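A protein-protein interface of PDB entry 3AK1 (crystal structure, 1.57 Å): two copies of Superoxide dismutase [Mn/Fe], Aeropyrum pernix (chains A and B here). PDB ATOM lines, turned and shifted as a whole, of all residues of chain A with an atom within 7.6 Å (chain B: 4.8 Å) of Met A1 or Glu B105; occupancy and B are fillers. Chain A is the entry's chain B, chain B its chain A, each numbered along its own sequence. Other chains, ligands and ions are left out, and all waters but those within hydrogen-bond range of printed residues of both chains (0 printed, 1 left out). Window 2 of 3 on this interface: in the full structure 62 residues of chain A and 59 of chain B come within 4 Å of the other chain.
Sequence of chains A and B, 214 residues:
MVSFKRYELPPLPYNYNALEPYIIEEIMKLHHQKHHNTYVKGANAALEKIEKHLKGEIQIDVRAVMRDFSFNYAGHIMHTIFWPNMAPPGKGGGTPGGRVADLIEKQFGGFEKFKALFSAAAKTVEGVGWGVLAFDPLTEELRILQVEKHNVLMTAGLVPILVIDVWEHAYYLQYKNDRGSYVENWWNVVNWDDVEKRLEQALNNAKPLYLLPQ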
ATOM      1  N   MET A   1     -30.399  18.585 -23.078  1.00  0.00           N
ATOM      2  CA  MET A   1     -30.241  19.555 -21.954  1.00  0.00           C
ATOM      3  C   MET A   1     -30.183  18.848 -20.601  1.00  0.00           C
ATOM      4  O   MET A   1     -30.919  17.889 -20.351  1.00  0.00           O
ATOM      5  CB  MET A   1     -31.386  20.572 -21.963  1.00  0.00           C
ATOM      6  CG  MET A   1     -31.101  21.851 -21.189  1.00  0.00           C
ATOM      7  SD  MET A   1     -32.398  23.097 -21.387  1.00  0.00           S
ATOM      8  CE  MET A   1     -33.519  22.632 -20.074  1.00  0.00           C
ATOM      9  N   VAL A   2     -29.296  19.331 -19.735  1.00  0.00           N
ATOM     10  CA  VAL A   2     -29.196  18.855 -18.358  1.00  0.00           C
ATOM     11  C   VAL A   2     -29.506  20.000 -17.385  1.00  0.00           C
ATOM     12  O   VAL A   2     -29.942  19.768 -16.251  1.00  0.00           O
ATOM     13  CB  VAL A   2     -27.795  18.284 -18.045  1.00  0.00           C
ATOM     14  CG1 VAL A   2     -27.842  17.531 -16.750  1.00  0.00           C
ATOM     15  CG2 VAL A   2     -27.313  17.360 -19.157  1.00  0.00           C
ATOM     16  N   SER A   3     -29.268  21.228 -17.846  1.00  0.00           N
ATOM     17  CA  SER A   3     -29.581  22.457 -17.110  1.00  0.00           C
ATOM     18  C   SER A   3     -28.431  22.930 -16.205  1.00  0.00           C
ATOM     19  O   SER A   3     -27.316  23.129 -16.700  1.00  0.00           O
ATOM     20  CB  SER A   3     -30.906  22.331 -16.354  1.00  0.00           C
ATOM     21  OG  SER A   3     -31.951  21.931 -17.231  1.00  0.00           O
ATOM     22  N   PHE A   4     -28.685  23.105 -14.902  1.00  0.00           N
ATOM     23  CA  PHE A   4     -27.708  23.769 -14.022  1.00  0.00           C
ATOM     24  C   PHE A   4     -27.315  23.042 -12.733  1.00  0.00           C
ATOM     25  O   PHE A   4     -28.145  22.410 -12.071  1.00  0.00           O
ATOM     26  CB  PHE A   4     -28.162  25.206 -13.696  1.00  0.00           C
ATOM     27  CG  PHE A   4     -29.107  25.308 -12.517  1.00  0.00           C
ATOM     28  CD1 PHE A   4     -28.623  25.623 -11.245  1.00  0.00           C
ATOM     29  CD2 PHE A   4     -30.474  25.106 -12.679  1.00  0.00           C
ATOM     30  CE1 PHE A   4     -29.485  25.737 -10.158  1.00  0.00           C
ATOM     31  CE2 PHE A   4     -31.347  25.208 -11.590  1.00  0.00           C
ATOM     32  CZ  PHE A   4     -30.852  25.525 -10.331  1.00  0.00           C
ATOM     33  N   ILE A  50     -34.593  30.466 -15.173  1.00  0.00           N
ATOM     34  CA  ILE A  50     -33.976  30.448 -16.497  1.00  0.00           C
ATOM     35  C   ILE A  50     -34.195  29.079 -17.146  1.00  0.00           C
ATOM     36  O   ILE A  50     -34.372  28.985 -18.359  1.00  0.00           O
ATOM     37  CB  ILE A  50     -32.456  30.796 -16.449  1.00  0.00           C
ATOM     38  CG1 ILE A  50     -32.222  32.227 -15.928  1.00  0.00           C
ATOM     39  CG2 ILE A  50     -31.787  30.591 -17.809  1.00  0.00           C
ATOM     40  CD1 ILE A  50     -32.594  33.360 -16.879  1.00  0.00           C
ATOM     41  N   GLU A  51     -34.172  28.033 -16.325  1.00  0.00           N
ATOM     42  CA  GLU A  51     -34.442  26.664 -16.766  1.00  0.00           C
ATOM     43  C   GLU A  51     -35.822  26.561 -17.385  1.00  0.00           C
ATOM     44  O   GLU A  51     -35.971  26.112 -18.528  1.00  0.00           O
ATOM     45  CB  GLU A  51     -34.400  25.719 -15.577  1.00  0.00           C
ATOM     46  CG  GLU A  51     -33.098  25.015 -15.356  1.00  0.00           C
ATOM     47  CD  GLU A  51     -33.327  23.632 -14.784  1.00  0.00           C
ATOM     48  OE1 GLU A  51     -34.128  22.875 -15.369  1.00  0.00           O
ATOM     49  OE2 GLU A  51     -32.718  23.296 -13.750  1.00  0.00           O
ATOM     50  N   LYS A  52     -36.826  26.973 -16.615  1.00  0.00           N
ATOM     51  CA  LYS A  52     -38.218  26.913 -17.051  1.00  0.00           C
ATOM     52  C   LYS A  52     -38.429  27.726 -18.325  1.00  0.00           C
ATOM     53  O   LYS A  52     -39.198  27.330 -19.195  1.00  0.00           O
ATOM     54  CB  LYS A  52     -39.155  27.391 -15.940  1.00  0.00           C
ATOM     55  CG  LYS A  52     -39.174  26.496 -14.704  1.00  0.00           C
ATOM     56  CD  LYS A  52     -40.075  27.081 -13.629  1.00  0.00           C
ATOM     57  CE  LYS A  52     -40.339  26.087 -12.504  1.00  0.00           C
ATOM     58  NZ  LYS A  52     -41.307  25.021 -12.918  1.00  0.00           N
ATOM     59  N   HIS A  53     -37.721  28.848 -18.436  1.00  0.00           N
ATOM     60  CA  HIS A  53     -37.750  29.685 -19.633  1.00  0.00           C
ATOM     61  C   HIS A  53     -37.210  28.941 -20.857  1.00  0.00           C
ATOM     62  O   HIS A  53     -37.806  28.984 -21.938  1.00  0.00           O
ATOM     63  CB  HIS A  53     -36.939  30.964 -19.390  1.00  0.00           C
ATOM     64  CG  HIS A  53     -36.770  31.815 -20.608  1.00  0.00           C
ATOM     65  ND1 HIS A  53     -37.753  32.670 -21.060  1.00  0.00           N
ATOM     66  CD2 HIS A  53     -35.733  31.947 -21.467  1.00  0.00           C
ATOM     67  CE1 HIS A  53     -37.327  33.290 -22.146  1.00  0.00           C
ATOM     68  NE2 HIS A  53     -36.107  32.866 -22.417  1.00  0.00           N
ATOM     69  N   LEU A  54     -36.080  28.261 -20.678  1.00  0.00           N
ATOM     70  CA  LEU A  54     -35.429  27.532 -21.766  1.00  0.00           C
ATOM     71  C   LEU A  54     -36.264  26.342 -22.251  1.00  0.00           C
ATOM     72  O   LEU A  54     -36.148  25.927 -23.401  1.00  0.00           O
ATOM     73  CB  LEU A  54     -34.029  27.070 -21.346  1.00  0.00           C
ATOM     74  CG  LEU A  54     -32.982  28.171 -21.124  1.00  0.00           C
ATOM     75  CD1 LEU A  54     -31.793  27.616 -20.366  1.00  0.00           C
ATOM     76  CD2 LEU A  54     -32.542  28.794 -22.438  1.00  0.00           C
ATOM     77  N   LYS A  55     -37.098  25.809 -21.361  1.00  0.00           N
ATOM     78  CA  LYS A  55     -38.016  24.714 -21.688  1.00  0.00           C
ATOM     79  C   LYS A  55     -39.309  25.204 -22.363  1.00  0.00           C
ATOM     80  O   LYS A  55     -40.135  24.394 -22.794  1.00  0.00           O
ATOM     81  CB  LYS A  55     -38.354  23.919 -20.429  1.00  0.00           C
ATOM     82  CG  LYS A  55     -37.177  23.186 -19.817  1.00  0.00           C
ATOM     83  CD  LYS A  55     -37.611  22.397 -18.608  1.00  0.00           C
ATOM     84  CE  LYS A  55     -36.433  21.695 -17.957  1.00  0.00           C
ATOM     85  NZ  LYS A  55     -36.879  20.869 -16.799  1.00  0.00           N
ATOM     86  N   GLY A  56     -39.482  26.521 -22.453  1.00  0.00           N
ATOM     87  CA  GLY A  56     -40.657  27.118 -23.100  1.00  0.00           C
ATOM     88  C   GLY A  56     -41.880  27.091 -22.206  1.00  0.00           C
ATOM     89  O   GLY A  56     -43.005  27.350 -22.652  1.00  0.00           O
ATOM     90  N   ALA B 101     -19.585  24.229 -27.513  1.00  0.00           N
ATOM     91  CA  ALA B 101     -20.809  23.635 -28.053  1.00  0.00           C
ATOM     92  C   ALA B 101     -21.383  22.606 -27.095  1.00  0.00           C
ATOM     93  O   ALA B 101     -22.596  22.533 -26.913  1.00  0.00           O
ATOM     94  CB  ALA B 101     -20.554  23.012 -29.419  1.00  0.00           C
ATOM     95  N   ASP B 102     -20.507  21.825 -26.465  1.00  0.00           N
ATOM     96  CA  ASP B 102     -20.940  20.792 -25.538  1.00  0.00           C
ATOM     97  C   ASP B 102     -21.672  21.410 -24.353  1.00  0.00           C
ATOM     98  O   ASP B 102     -22.773  20.979 -24.009  1.00  0.00           O
ATOM     99  CB  ASP B 102     -19.752  19.948 -25.063  1.00  0.00           C
ATOM    100  CG  ASP B 102     -20.182  18.768 -24.199  1.00  0.00           C
ATOM    101  OD1 ASP B 102     -20.962  17.921 -24.687  1.00  0.00           O
ATOM    102  OD2 ASP B 102     -19.738  18.687 -23.031  1.00  0.00           O
ATOM    103  N   LEU B 103     -21.060  22.422 -23.738  1.00  0.00           N
ATOM    104  CA  LEU B 103     -21.663  23.095 -22.584  1.00  0.00           C
ATOM    105  C   LEU B 103     -22.947  23.819 -22.964  1.00  0.00           C
ATOM    106  O   LEU B 103     -23.909  23.803 -22.208  1.00  0.00           O
ATOM    107  CB  LEU B 103     -20.674  24.063 -21.921  1.00  0.00           C
ATOM    108  CG  LEU B 103     -19.560  23.448 -21.070  1.00  0.00           C
ATOM    109  CD1 LEU B 103     -18.720  24.540 -20.421  1.00  0.00           C
ATOM    110  CD2 LEU B 103     -20.108  22.512 -19.998  1.00  0.00           C
ATOM    111  N   ILE B 104     -22.958  24.438 -24.142  1.00  0.00           N
ATOM    112  CA  ILE B 104     -24.160  25.087 -24.661  1.00  0.00           C
ATOM    113  C   ILE B 104     -25.304  24.077 -24.832  1.00  0.00           C
ATOM    114  O   ILE B 104     -26.454  24.365 -24.467  1.00  0.00           O
ATOM    115  CB  ILE B 104     -23.856  25.865 -25.969  1.00  0.00           C
ATOM    116  CG1 ILE B 104     -23.164  27.195 -25.645  1.00  0.00           C
ATOM    117  CG2 ILE B 104     -25.119  26.109 -26.784  1.00  0.00           C
ATOM    118  CD1 ILE B 104     -22.621  27.928 -26.857  1.00  0.00           C
ATOM    119  N   GLU B 105     -24.978  22.898 -25.368  1.00  0.00           N
ATOM    120  CA  GLU B 105     -25.963  21.832 -25.529  1.00  0.00           C
ATOM    121  C   GLU B 105     -26.504  21.357 -24.182  1.00  0.00           C
ATOM    122  O   GLU B 105     -27.718  21.238 -24.008  1.00  0.00           O
ATOM    123  CB  GLU B 105     -25.377  20.655 -26.323  1.00  0.00           C
ATOM    124  CG  GLU B 105     -26.367  19.522 -26.611  1.00  0.00           C
ATOM    125  CD  GLU B 105     -27.533  19.940 -27.507  1.00  0.00           C
ATOM    126  OE1 GLU B 105     -28.634  19.365 -27.350  1.00  0.00           O
ATOM    127  OE2 GLU B 105     -27.350  20.828 -28.371  1.00  0.00           O
ATOM    128  N   LYS B 106     -25.608  21.106 -23.235  1.00  0.00           N
ATOM    129  CA  LYS B 106     -25.984  20.556 -21.935  1.00  0.00           C
ATOM    130  C   LYS B 106     -26.750  21.512 -21.037  1.00  0.00           C
ATOM    131  O   LYS B 106     -27.555  21.076 -20.213  1.00  0.00           O
ATOM    132  CB  LYS B 106     -24.745  20.048 -21.201  1.00  0.00           C
ATOM    133  CG  LYS B 106     -24.266  18.707 -21.722  1.00  0.00           C
ATOM    134  CD  LYS B 106     -22.894  18.360 -21.194  1.00  0.00           C
ATOM    135  CE  LYS B 106     -22.468  17.005 -21.718  1.00  0.00           C
ATOM    136  NZ  LYS B 106     -21.077  16.680 -21.319  1.00  0.00           N
ATOM    137  N   GLN B 107     -26.516  22.809 -21.204  1.00  0.00           N
ATOM    138  CA  GLN B 107     -27.055  23.792 -20.276  1.00  0.00           C
ATOM    139  C   GLN B 107     -28.219  24.582 -20.823  1.00  0.00           C
ATOM    140  O   GLN B 107     -29.184  24.835 -20.099  1.00  0.00           O
ATOM    141  CB  GLN B 107     -25.962  24.753 -19.854  1.00  0.00           C
ATOM    142  CG  GLN B 107     -24.823  24.081 -19.136  1.00  0.00           C
ATOM    143  CD  GLN B 107     -23.931  25.085 -18.533  1.00  0.00           C
ATOM    144  OE1 GLN B 107     -22.751  25.167 -18.870  1.00  0.00           O
ATOM    145  NE2 GLN B 107     -24.492  25.906 -17.641  1.00  0.00           N
ATOM    146  N   PHE B 108     -28.121  24.972 -22.090  1.00  0.00           N
ATOM    147  CA  PHE B 108     -29.129  25.832 -22.705  1.00  0.00           C
ATOM    148  C   PHE B 108     -30.039  25.075 -23.665  1.00  0.00           C
ATOM    149  O   PHE B 108     -31.037  25.618 -24.141  1.00  0.00           O
ATOM    150  CB  PHE B 108     -28.455  27.033 -23.386  1.00  0.00           C
ATOM    151  CG  PHE B 108     -27.543  27.809 -22.467  1.00  0.00           C
ATOM    152  CD1 PHE B 108     -28.073  28.579 -21.432  1.00  0.00           C
ATOM    153  CD2 PHE B 108     -26.161  27.754 -22.622  1.00  0.00           C
ATOM    154  CE1 PHE B 108     -27.238  29.289 -20.566  1.00  0.00           C
ATOM    155  CE2 PHE B 108     -25.311  28.468 -21.768  1.00  0.00           C
ATOM    156  CZ  PHE B 108     -25.852  29.236 -20.737  1.00  0.00           C
ATOM    157  N   GLY B 109     -29.697  23.815 -23.927  1.00  0.00           N
ATOM    158  CA  GLY B 109     -30.438  22.987 -24.878  1.00  0.00           C
ATOM    159  C   GLY B 109     -30.079  23.279 -26.321  1.00  0.00           C
ATOM    160  O   GLY B 109     -30.918  23.159 -27.224  1.00  0.00           O
ATOM    161  N   GLY B 110     -28.834  23.675 -26.553  1.00  0.00           N
ATOM    162  CA  GLY B 110     -28.360  23.893 -27.914  1.00  0.00           C
ATOM    163  C   GLY B 110     -28.113  25.337 -28.279  1.00  0.00           C
ATOM    164  O   GLY B 110     -28.468  26.257 -27.527  1.00  0.00           O
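The side-chain sulfur (SD) of Met A1 lies close to the backbone NH (N) of Gly B109 (3.8 Å).
The backbone carbonyl oxygen of Lys B106 is in hydrogen-bond range of the backbone NH of Ser A3, at 2.9 Å.
The backbone NH (N) of Val A2 lies within hydrogen-bond range of the backbone carbonyl oxygen (O) of Lys B106 (2.5 Å).
The backbone carbonyl oxygen (O) of Ile B104 lies within hydrogen-bond range of the backbone NH (N) of Gly B109 (3.3 Å).
The side-chain carboxylate of Asp B102 lies within salt-bridge range of the side-chain amino group of Lys B106.
The side-chain hydroxyl of Ser A3 is in hydrogen-bond range of the side-chain carboxylate of Glu A51, at 3.0 Å.
Among the printed residues, pairs that only touch across the chains: Met A1 with Lys B106 (3.5 Å), Ser A3 with Gln B107 (3.6 Å), Met A1 with Glu B105 (3.7 Å), Met A1 with Gln B107 (3.7 Å), Leu A54 with Gln B107 (3.8 Å), Met A1 with Phe B108 (3.8 Å) and Leu A54 with Phe B108 (3.9 Å).
Of the printed residues of chain B, Met A1 touches Glu B105 (3.7 Å), Lys B106 (3.5 Å), Gln B107 (3.7 Å), Phe B108 (3.8 Å) and Gly B109 (3.7 Å).
Of the printed residues of chain A, Glu B105 touches Met A1 (3.7 Å).
Printed residues of chain B within 4 Å of Val A2: Lys B106 (2.5 Å).
Printed residues of chain A within 4 Å of Phe B108: Met A1 (3.8 Å) and Leu A54 (3.9 Å).
Printed residues of chain A within 4 Å of Gly B109: Met A1.
Ile B104 touches none of the printed residues of chain A.
The nearest printed residue of chain B that does not touch Met A1 is Gly B110 (6.1 Å).
The nearest printed residue of chain B that does not touch Leu A54 is Gly B109 (5.6 Å).
Hydrophobic or aromatic side chains of chain B within 4 Å of the printed part of chain A: Phe B108.
Along chain B the printed residues that touch a printed residue of chain A span positions 105 to 109.
Of the 11 printed residues of chain A, 4 touch a printed residue of chain B.
Among the printed residues, no Asp or Glu carboxylate lies within 4 Å of a Lys or Arg side-chain nitrogen of the other chain.
No position is printed for both chains.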
